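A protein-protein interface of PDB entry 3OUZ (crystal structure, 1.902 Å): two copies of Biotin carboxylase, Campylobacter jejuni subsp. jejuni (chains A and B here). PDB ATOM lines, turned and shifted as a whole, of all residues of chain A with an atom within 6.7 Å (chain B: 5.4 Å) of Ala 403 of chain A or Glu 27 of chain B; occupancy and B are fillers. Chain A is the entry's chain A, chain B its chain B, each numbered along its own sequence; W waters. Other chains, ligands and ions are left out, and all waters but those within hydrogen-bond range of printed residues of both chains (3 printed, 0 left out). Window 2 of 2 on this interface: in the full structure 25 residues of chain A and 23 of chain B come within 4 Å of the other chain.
Of the 17 printed residues of chain A, 6 touch a printed residue of chain B. Hydrophobic or aromatic side chains of chain A within 4 Å of the printed part of chain B: Ala 364, Ala 403 and Val 407. Among the printed residues, Asp or Glu carboxylates within 4 Å of a Lys or Arg side-chain nitrogen of the other chain: Lys 404 of chain A with Glu 27 of chain B (2.5 Å).
Water W3 lies within hydrogen-bond range of the side-chain carboxylate of Glu 27 of chain B (2.7 Å) and the backbone carbonyl oxygen of Lys 404 of chain A (2.9 Å). Water W2 bridges OE2 of Glu 27 of chain B and NZ of Lys 404 of chain A. Water W1 lies within hydrogen-bond range of the guanidinium group of Arg 366 of chain A, the side-chain carboxylate of Glu 27 of chain B, the side-chain amino group of Lys 404 of chain A and the side-chain carboxylate of Asp 311 of chain B.
The side-chain amino group of Lys 404 of chain A lies within salt-bridge range of the side-chain carboxylate of Glu 27 of chain B.
The side-chain amino group (NZ) of Lys 404 of chain A lies within hydrogen-bond range of the backbone carbonyl oxygen (O) of Arg 366 of chain A, at 2.8 Å. The side-chain hydroxyl of Thr 24 of chain B lies within hydrogen-bond range of the side-chain carboxylate of Asp 311 of chain B (2.6 Å).
Printed residues of chain B within 4 Å of Arg 366 of chain A: Asp 311. Ala 403 of chain A touches one residue of chain B. Printed residues of chain B within 4 Å of Lys 404 of chain A: Glu 27 (2.5 Å). Leu 22 of chain B touches none of the printed residues of chain A. Printed residues of chain A within 4 Å of Arg 23 of chain B: Ala 364 and Gly 365. The nearest printed residue of chain B that does not touch Ala 403 of chain A is Lys 26 of chain B (5.7 Å). The nearest printed residue of chain B that does not touch Lys 404 of chain A is Asp 311 of chain B (6.2 Å).
Among the printed residues, merely in contact across the chains: Ala 364 of chain A with Arg 23 of chain B (3.6 Å), Arg 366 of chain A with Asp 311 of chain B (3.7 Å), Ala 403 of chain A with Glu 27 of chain B (3.7 Å), Val 407 of chain A with Glu 27 of chain B (3.8 Å), Gly 365 of chain A with Arg 23 of chain B (3.9 Å) and Val 407 of chain A with Lys 26 of chain B (3.9 Å).
No position is printed for both chains.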
ATOM      1  N   ILE A 338     -22.351 -14.737  17.412  1.00  0.00           N
ATOM      2  CA  ILE A 338     -21.451 -15.712  18.020  1.00  0.00           C
ATOM      3  C   ILE A 338     -20.397 -16.008  16.992  1.00  0.00           C
ATOM      4  O   ILE A 338     -20.705 -16.119  15.798  1.00  0.00           O
ATOM      5  CB  ILE A 338     -22.200 -17.044  18.342  1.00  0.00           C
ATOM      6  CG1 ILE A 338     -23.413 -16.760  19.235  1.00  0.00           C
ATOM      7  CG2 ILE A 338     -21.231 -18.080  18.997  1.00  0.00           C
ATOM      8  CD1 ILE A 338     -24.280 -18.025  19.558  1.00  0.00           C
ATOM      9  N   ALA A 364     -22.482 -20.630   4.029  1.00  0.00           N
ATOM     10  CA  ALA A 364     -22.889 -19.305   3.600  1.00  0.00           C
ATOM     11  C   ALA A 364     -24.310 -19.151   4.076  1.00  0.00           C
ATOM     12  O   ALA A 364     -24.759 -19.891   4.935  1.00  0.00           O
ATOM     13  CB  ALA A 364     -22.791 -19.161   2.068  1.00  0.00           C
ATOM     14  N   GLY A 365     -25.024 -18.184   3.538  1.00  0.00           N
ATOM     15  CA  GLY A 365     -26.399 -18.001   3.947  1.00  0.00           C
ATOM     16  C   GLY A 365     -26.580 -16.648   4.593  1.00  0.00           C
ATOM     17  O   GLY A 365     -25.623 -15.899   4.787  1.00  0.00           O
ATOM     18  N   ARG A 366     -27.825 -16.346   4.922  1.00  0.00           N
ATOM     19  CA  ARG A 366     -28.186 -15.071   5.505  1.00  0.00           C
ATOM     20  C   ARG A 366     -27.486 -14.896   6.864  1.00  0.00           C
ATOM     21  O   ARG A 366     -27.589 -15.762   7.735  1.00  0.00           O
ATOM     22  CB  ARG A 366     -29.714 -15.068   5.663  1.00  0.00           C
ATOM     23  CG  ARG A 366     -30.295 -13.915   6.435  1.00  0.00           C
ATOM     24  CD  ARG A 366     -31.841 -13.984   6.373  1.00  0.00           C
ATOM     25  NE  ARG A 366     -32.413 -12.981   7.256  1.00  0.00           N
ATOM     26  CZ  ARG A 366     -32.727 -13.189   8.525  1.00  0.00           C
ATOM     27  NH1 ARG A 366     -32.558 -14.384   9.074  1.00  0.00           N
ATOM     28  NH2 ARG A 366     -33.209 -12.191   9.245  1.00  0.00           N
ATOM     29  N   VAL A 368     -24.476 -15.117   7.813  1.00  0.00           N
ATOM     30  CA  VAL A 368     -23.386 -16.034   8.096  1.00  0.00           C
ATOM     31  C   VAL A 368     -22.144 -15.467   7.457  1.00  0.00           C
ATOM     32  O   VAL A 368     -22.153 -15.151   6.276  1.00  0.00           O
ATOM     33  CB  VAL A 368     -23.676 -17.423   7.500  1.00  0.00           C
ATOM     34  CG1 VAL A 368     -22.438 -18.340   7.619  1.00  0.00           C
ATOM     35  CG2 VAL A 368     -24.861 -18.041   8.217  1.00  0.00           C
ATOM     36  N   ARG A 398     -30.109 -14.987  21.191  1.00  0.00           N
ATOM     37  CA  ARG A 398     -29.026 -15.970  21.384  1.00  0.00           C
ATOM     38  C   ARG A 398     -29.391 -17.380  20.903  1.00  0.00           C
ATOM     39  O   ARG A 398     -28.597 -18.038  20.226  1.00  0.00           O
ATOM     40  CB  ARG A 398     -28.595 -16.028  22.850  1.00  0.00           C
ATOM     41  CG  ARG A 398     -27.365 -16.947  23.100  1.00  0.00           C
ATOM     42  CD  ARG A 398     -26.777 -16.694  24.527  1.00  0.00           C
ATOM     43  NE  ARG A 398     -25.463 -17.310  24.715  1.00  0.00           N
ATOM     44  CZ  ARG A 398     -25.276 -18.485  25.319  1.00  0.00           C
ATOM     45  NH1 ARG A 398     -26.325 -19.175  25.766  1.00  0.00           N
ATOM     46  NH2 ARG A 398     -24.047 -18.973  25.464  1.00  0.00           N
ATOM     47  N   ASN A 399     -30.574 -17.871  21.270  1.00  0.00           N
ATOM     48  CA  ASN A 399     -30.954 -19.220  20.828  1.00  0.00           C
ATOM     49  C   ASN A 399     -31.028 -19.337  19.307  1.00  0.00           C
ATOM     50  O   ASN A 399     -30.638 -20.359  18.730  1.00  0.00           O
ATOM     51  CB  ASN A 399     -32.277 -19.663  21.484  1.00  0.00           C
ATOM     52  CG  ASN A 399     -32.086 -20.011  22.939  1.00  0.00           C
ATOM     53  OD1 ASN A 399     -31.000 -20.432  23.334  1.00  0.00           O
ATOM     54  ND2 ASN A 399     -33.118 -19.822  23.745  1.00  0.00           N
ATOM     55  N   LYS A 400     -31.531 -18.294  18.653  1.00  0.00           N
ATOM     56  CA  LYS A 400     -31.535 -18.274  17.191  1.00  0.00           C
ATOM     57  C   LYS A 400     -30.128 -18.262  16.627  1.00  0.00           C
ATOM     58  O   LYS A 400     -29.863 -18.891  15.594  1.00  0.00           O
ATOM     59  CB  LYS A 400     -32.340 -17.081  16.642  1.00  0.00           C
ATOM     60  CG  LYS A 400     -33.842 -17.280  16.848  1.00  0.00           C
ATOM     61  CD  LYS A 400     -34.654 -16.057  16.400  1.00  0.00           C
ATOM     62  CE  LYS A 400     -36.145 -16.407  16.446  1.00  0.00           C
ATOM     63  NZ  LYS A 400     -36.989 -15.275  15.979  1.00  0.00           N
ATOM     64  N   ALA A 401     -29.221 -17.534  17.275  1.00  0.00           N
ATOM     65  CA  ALA A 401     -27.833 -17.531  16.820  1.00  0.00           C
ATOM     66  C   ALA A 401     -27.181 -18.901  17.026  1.00  0.00           C
ATOM     67  O   ALA A 401     -26.417 -19.368  16.181  1.00  0.00           O
ATOM     68  CB  ALA A 401     -27.003 -16.415  17.528  1.00  0.00           C
ATOM     69  N   ILE A 402     -27.461 -19.545  18.156  1.00  0.00           N
ATOM     70  CA  ILE A 402     -26.912 -20.885  18.368  1.00  0.00           C
ATOM     71  C   ILE A 402     -27.445 -21.837  17.270  1.00  0.00           C
ATOM     72  O   ILE A 402     -26.693 -22.632  16.698  1.00  0.00           O
ATOM     73  CB  ILE A 402     -27.252 -21.414  19.792  1.00  0.00           C
ATOM     74  CG1 ILE A 402     -26.471 -20.627  20.850  1.00  0.00           C
ATOM     75  CG2 ILE A 402     -26.956 -22.900  19.904  1.00  0.00           C
ATOM     76  CD1 ILE A 402     -26.931 -20.925  22.284  1.00  0.00           C
ATOM     77  N   ALA A 403     -28.733 -21.742  16.958  1.00  0.00           N
ATOM     78  CA  ALA A 403     -29.292 -22.607  15.903  1.00  0.00           C
ATOM     79  C   ALA A 403     -28.652 -22.346  14.531  1.00  0.00           C
ATOM     80  O   ALA A 403     -28.388 -23.285  13.781  1.00  0.00           O
ATOM     81  CB  ALA A 403     -30.830 -22.488  15.829  1.00  0.00           C
ATOM     82  N   LYS A 404     -28.408 -21.076  14.207  1.00  0.00           N
ATOM     83  CA  LYS A 404     -27.773 -20.728  12.940  1.00  0.00           C
ATOM     84  C   LYS A 404     -26.307 -21.208  12.906  1.00  0.00           C
ATOM     85  O   LYS A 404     -25.825 -21.675  11.867  1.00  0.00           O
ATOM     86  CB  LYS A 404     -27.864 -19.206  12.684  1.00  0.00           C
ATOM     87  CG  LYS A 404     -27.063 -18.741  11.487  1.00  0.00           C
ATOM     88  CD  LYS A 404     -27.390 -17.272  11.083  1.00  0.00           C
ATOM     89  CE  LYS A 404     -28.789 -17.137  10.510  1.00  0.00           C
ATOM     90  NZ  LYS A 404     -28.954 -17.776   9.165  1.00  0.00           N
ATOM     91  N   MET A 405     -25.610 -21.111  14.040  1.00  0.00           N
ATOM     92  CA  MET A 405     -24.225 -21.604  14.139  1.00  0.00           C
ATOM     93  C   MET A 405     -24.152 -23.121  13.879  1.00  0.00           C
ATOM     94  O   MET A 405     -23.268 -23.595  13.161  1.00  0.00           O
ATOM     95  CB  MET A 405     -23.587 -21.236  15.495  1.00  0.00           C
ATOM     96  CG  MET A 405     -22.132 -21.740  15.658  1.00  0.00           C
ATOM     97  SD  MET A 405     -20.956 -20.913  14.288  1.00  0.00           S
ATOM     98  CE  MET A 405     -20.705 -19.180  15.206  1.00  0.00           C
ATOM     99  N   LYS A 406     -25.081 -23.882  14.444  1.00  0.00           N
ATOM    100  CA  LYS A 406     -25.074 -25.328  14.212  1.00  0.00           C
ATOM    101  C   LYS A 406     -25.296 -25.648  12.729  1.00  0.00           C
ATOM    102  O   LYS A 406     -24.594 -26.471  12.151  1.00  0.00           O
ATOM    103  CB  LYS A 406     -26.123 -26.053  15.065  1.00  0.00           C
ATOM    104  CG  LYS A 406     -26.128 -27.555  14.814  1.00  0.00           C
ATOM    105  CD  LYS A 406     -27.301 -28.261  15.473  1.00  0.00           C
ATOM    106  CE  LYS A 406     -27.276 -29.751  15.158  1.00  0.00           C
ATOM    107  NZ  LYS A 406     -27.355 -30.030  13.699  1.00  0.00           N
ATOM    108  N   VAL A 407     -26.260 -24.984  12.104  1.00  0.00           N
ATOM    109  CA  VAL A 407     -26.481 -25.205  10.672  1.00  0.00           C
ATOM    110  C   VAL A 407     -25.223 -24.853   9.851  1.00  0.00           C
ATOM    111  O   VAL A 407     -24.839 -25.606   8.960  1.00  0.00           O
ATOM    112  CB  VAL A 407     -27.736 -24.445  10.162  1.00  0.00           C
ATOM    113  CG1 VAL A 407     -27.754 -24.386   8.641  1.00  0.00           C
ATOM    114  CG2 VAL A 407     -29.004 -25.110  10.698  1.00  0.00           C
ATOM    115  N   ALA A 408     -24.588 -23.714  10.151  1.00  0.00           N
ATOM    116  CA  ALA A 408     -23.384 -23.282   9.436  1.00  0.00           C
ATOM    117  C   ALA A 408     -22.205 -24.226   9.677  1.00  0.00           C
ATOM    118  O   ALA A 408     -21.479 -24.583   8.744  1.00  0.00           O
ATOM    119  CB  ALA A 408     -22.998 -21.855   9.832  1.00  0.00           C
ATOM    120  N   MET A 428     -22.314 -26.098  20.794  1.00  0.00           N
ATOM    121  CA  MET A 428     -23.636 -25.539  20.454  1.00  0.00           C
ATOM    122  C   MET A 428     -24.759 -26.440  20.993  1.00  0.00           C
ATOM    123  O   MET A 428     -25.860 -25.975  21.227  1.00  0.00           O
ATOM    124  CB  MET A 428     -23.812 -25.349  18.931  1.00  0.00           C
ATOM    125  CG  MET A 428     -22.902 -24.251  18.308  1.00  0.00           C
ATOM    126  SD  MET A 428     -22.940 -22.498  19.168  1.00  0.00           S
ATOM    127  CE  MET A 428     -21.171 -22.621  20.019  1.00  0.00           C
ATOM    128  N   LEU B  22     -33.501 -24.878   2.303  1.00  0.00           N
ATOM    129  CA  LEU B  22     -33.043 -25.845   3.292  1.00  0.00           C
ATOM    130  C   LEU B  22     -32.429 -25.154   4.518  1.00  0.00           C
ATOM    131  O   LEU B  22     -32.684 -25.527   5.659  1.00  0.00           O
ATOM    132  CB  LEU B  22     -32.042 -26.816   2.643  1.00  0.00           C
ATOM    133  CG  LEU B  22     -31.351 -27.856   3.537  1.00  0.00           C
ATOM    134  CD1 LEU B  22     -30.933 -29.065   2.712  1.00  0.00           C
ATOM    135  CD2 LEU B  22     -30.124 -27.238   4.247  1.00  0.00           C
ATOM    136  N   ARG B  23     -31.619 -24.130   4.279  1.00  0.00           N
ATOM    137  CA  ARG B  23     -30.999 -23.428   5.388  1.00  0.00           C
ATOM    138  C   ARG B  23     -32.038 -22.890   6.355  1.00  0.00           C
ATOM    139  O   ARG B  23     -31.957 -23.138   7.548  1.00  0.00           O
ATOM    140  CB  ARG B  23     -30.076 -22.308   4.885  1.00  0.00           C
ATOM    141  CG  ARG B  23     -28.824 -22.835   4.201  1.00  0.00           C
ATOM    142  CD  ARG B  23     -27.996 -21.702   3.611  1.00  0.00           C
ATOM    143  NE  ARG B  23     -26.749 -22.202   3.050  1.00  0.00           N
ATOM    144  CZ  ARG B  23     -26.205 -21.748   1.926  1.00  0.00           C
ATOM    145  NH1 ARG B  23     -26.803 -20.791   1.237  1.00  0.00           N
ATOM    146  NH2 ARG B  23     -25.063 -22.260   1.493  1.00  0.00           N
ATOM    147  N   THR B  24     -33.020 -22.157   5.844  1.00  0.00           N
ATOM    148  CA  THR B  24     -34.031 -21.574   6.724  1.00  0.00           C
ATOM    149  C   THR B  24     -34.826 -22.663   7.446  1.00  0.00           C
ATOM    150  O   THR B  24     -35.098 -22.565   8.641  1.00  0.00           O
ATOM    151  CB  THR B  24     -34.972 -20.639   5.938  1.00  0.00           C
ATOM    152  OG1 THR B  24     -34.275 -19.420   5.701  1.00  0.00           O
ATOM    153  CG2 THR B  24     -36.226 -20.303   6.719  1.00  0.00           C
ATOM    154  N   ILE B  25     -35.186 -23.704   6.708  1.00  0.00           N
ATOM    155  CA  ILE B  25     -35.961 -24.814   7.289  1.00  0.00           C
ATOM    156  C   ILE B  25     -35.202 -25.471   8.449  1.00  0.00           C
ATOM    157  O   ILE B  25     -35.746 -25.649   9.546  1.00  0.00           O
ATOM    158  CB  ILE B  25     -36.313 -25.839   6.201  1.00  0.00           C
ATOM    159  CG1 ILE B  25     -37.291 -25.210   5.186  1.00  0.00           C
ATOM    160  CG2 ILE B  25     -36.944 -27.135   6.810  1.00  0.00           C
ATOM    161  CD1 ILE B  25     -37.357 -25.949   3.836  1.00  0.00           C
ATOM    162  N   LYS B  26     -33.943 -25.822   8.219  1.00  0.00           N
ATOM    163  CA  LYS B  26     -33.163 -26.440   9.280  1.00  0.00           C
ATOM    164  C   LYS B  26     -32.916 -25.478  10.458  1.00  0.00           C
ATOM    165  O   LYS B  26     -32.980 -25.885  11.609  1.00  0.00           O
ATOM    166  CB  LYS B  26     -31.854 -27.028   8.735  1.00  0.00           C
ATOM    167  CG  LYS B  26     -32.090 -28.106   7.670  1.00  0.00           C
ATOM    168  CD  LYS B  26     -30.825 -28.906   7.380  1.00  0.00           C
ATOM    169  CE  LYS B  26     -30.669 -30.074   8.369  1.00  0.00           C
ATOM    170  NZ  LYS B  26     -29.336 -30.716   8.206  1.00  0.00           N
ATOM    171  N   GLU B  27     -32.659 -24.205  10.182  1.00  0.00           N
ATOM    172  CA  GLU B  27     -32.479 -23.250  11.291  1.00  0.00           C
ATOM    173  C   GLU B  27     -33.713 -23.179  12.166  1.00  0.00           C
ATOM    174  O   GLU B  27     -33.603 -23.016  13.383  1.00  0.00           O
ATOM    175  CB  GLU B  27     -32.133 -21.851  10.768  1.00  0.00           C
ATOM    176  CG  GLU B  27     -30.697 -21.742  10.306  1.00  0.00           C
ATOM    177  CD  GLU B  27     -30.400 -20.419   9.604  1.00  0.00           C
ATOM    178  OE1 GLU B  27     -31.297 -19.544   9.538  1.00  0.00           O
ATOM    179  OE2 GLU B  27     -29.270 -20.268   9.094  1.00  0.00           O
ATOM    180  N   MET B  28     -34.891 -23.313  11.553  1.00  0.00           N
ATOM    181  CA  MET B  28     -36.132 -23.317  12.325  1.00  0.00           C
ATOM    182  C   MET B  28     -36.350 -24.623  13.090  1.00  0.00           C
ATOM    183  O   MET B  28     -37.333 -24.762  13.805  1.00  0.00           O
ATOM    184  CB  MET B  28     -37.346 -23.053  11.427  1.00  0.00           C
ATOM    185  CG  MET B  28     -37.348 -21.667  10.783  1.00  0.00           C
ATOM    186  SD  MET B  28     -38.859 -21.493   9.536  1.00  0.00           S
ATOM    187  CE  MET B  28     -40.246 -21.046  10.847  1.00  0.00           C
ATOM    188  N   GLY B  29     -35.454 -25.586  12.922  1.00  0.00           N
ATOM    189  CA  GLY B  29     -35.590 -26.848  13.637  1.00  0.00           C
ATOM    190  C   GLY B  29     -36.590 -27.791  12.987  1.00  0.00           C
ATOM    191  O   GLY B  29     -37.112 -28.692  13.637  1.00  0.00           O
ATOM    192  N   ASP B 311     -36.305 -12.673   7.022  1.00  0.00           N
ATOM    193  CA  ASP B 311     -36.125 -13.921   6.282  1.00  0.00           C
ATOM    194  C   ASP B 311     -37.466 -14.232   5.619  1.00  0.00           C
ATOM    195  O   ASP B 311     -38.408 -14.625   6.283  1.00  0.00           O
ATOM    196  CB  ASP B 311     -35.700 -15.074   7.237  1.00  0.00           C
ATOM    197  CG  ASP B 311     -35.475 -16.397   6.506  1.00  0.00           C
ATOM    198  OD1 ASP B 311     -36.071 -16.591   5.430  1.00  0.00           O
ATOM    199  OD2 ASP B 311     -34.727 -17.266   7.026  1.00  0.00           O
HETATM  200  O   HOH W   1     -31.833 -17.020   8.219  1.00  0.00           O
HETATM  201  O   HOH W   2     -28.265 -19.633   6.693  1.00  0.00           O
HETATM  202  O   HOH W   3     -26.757 -21.109   9.148  1.00  0.00           O
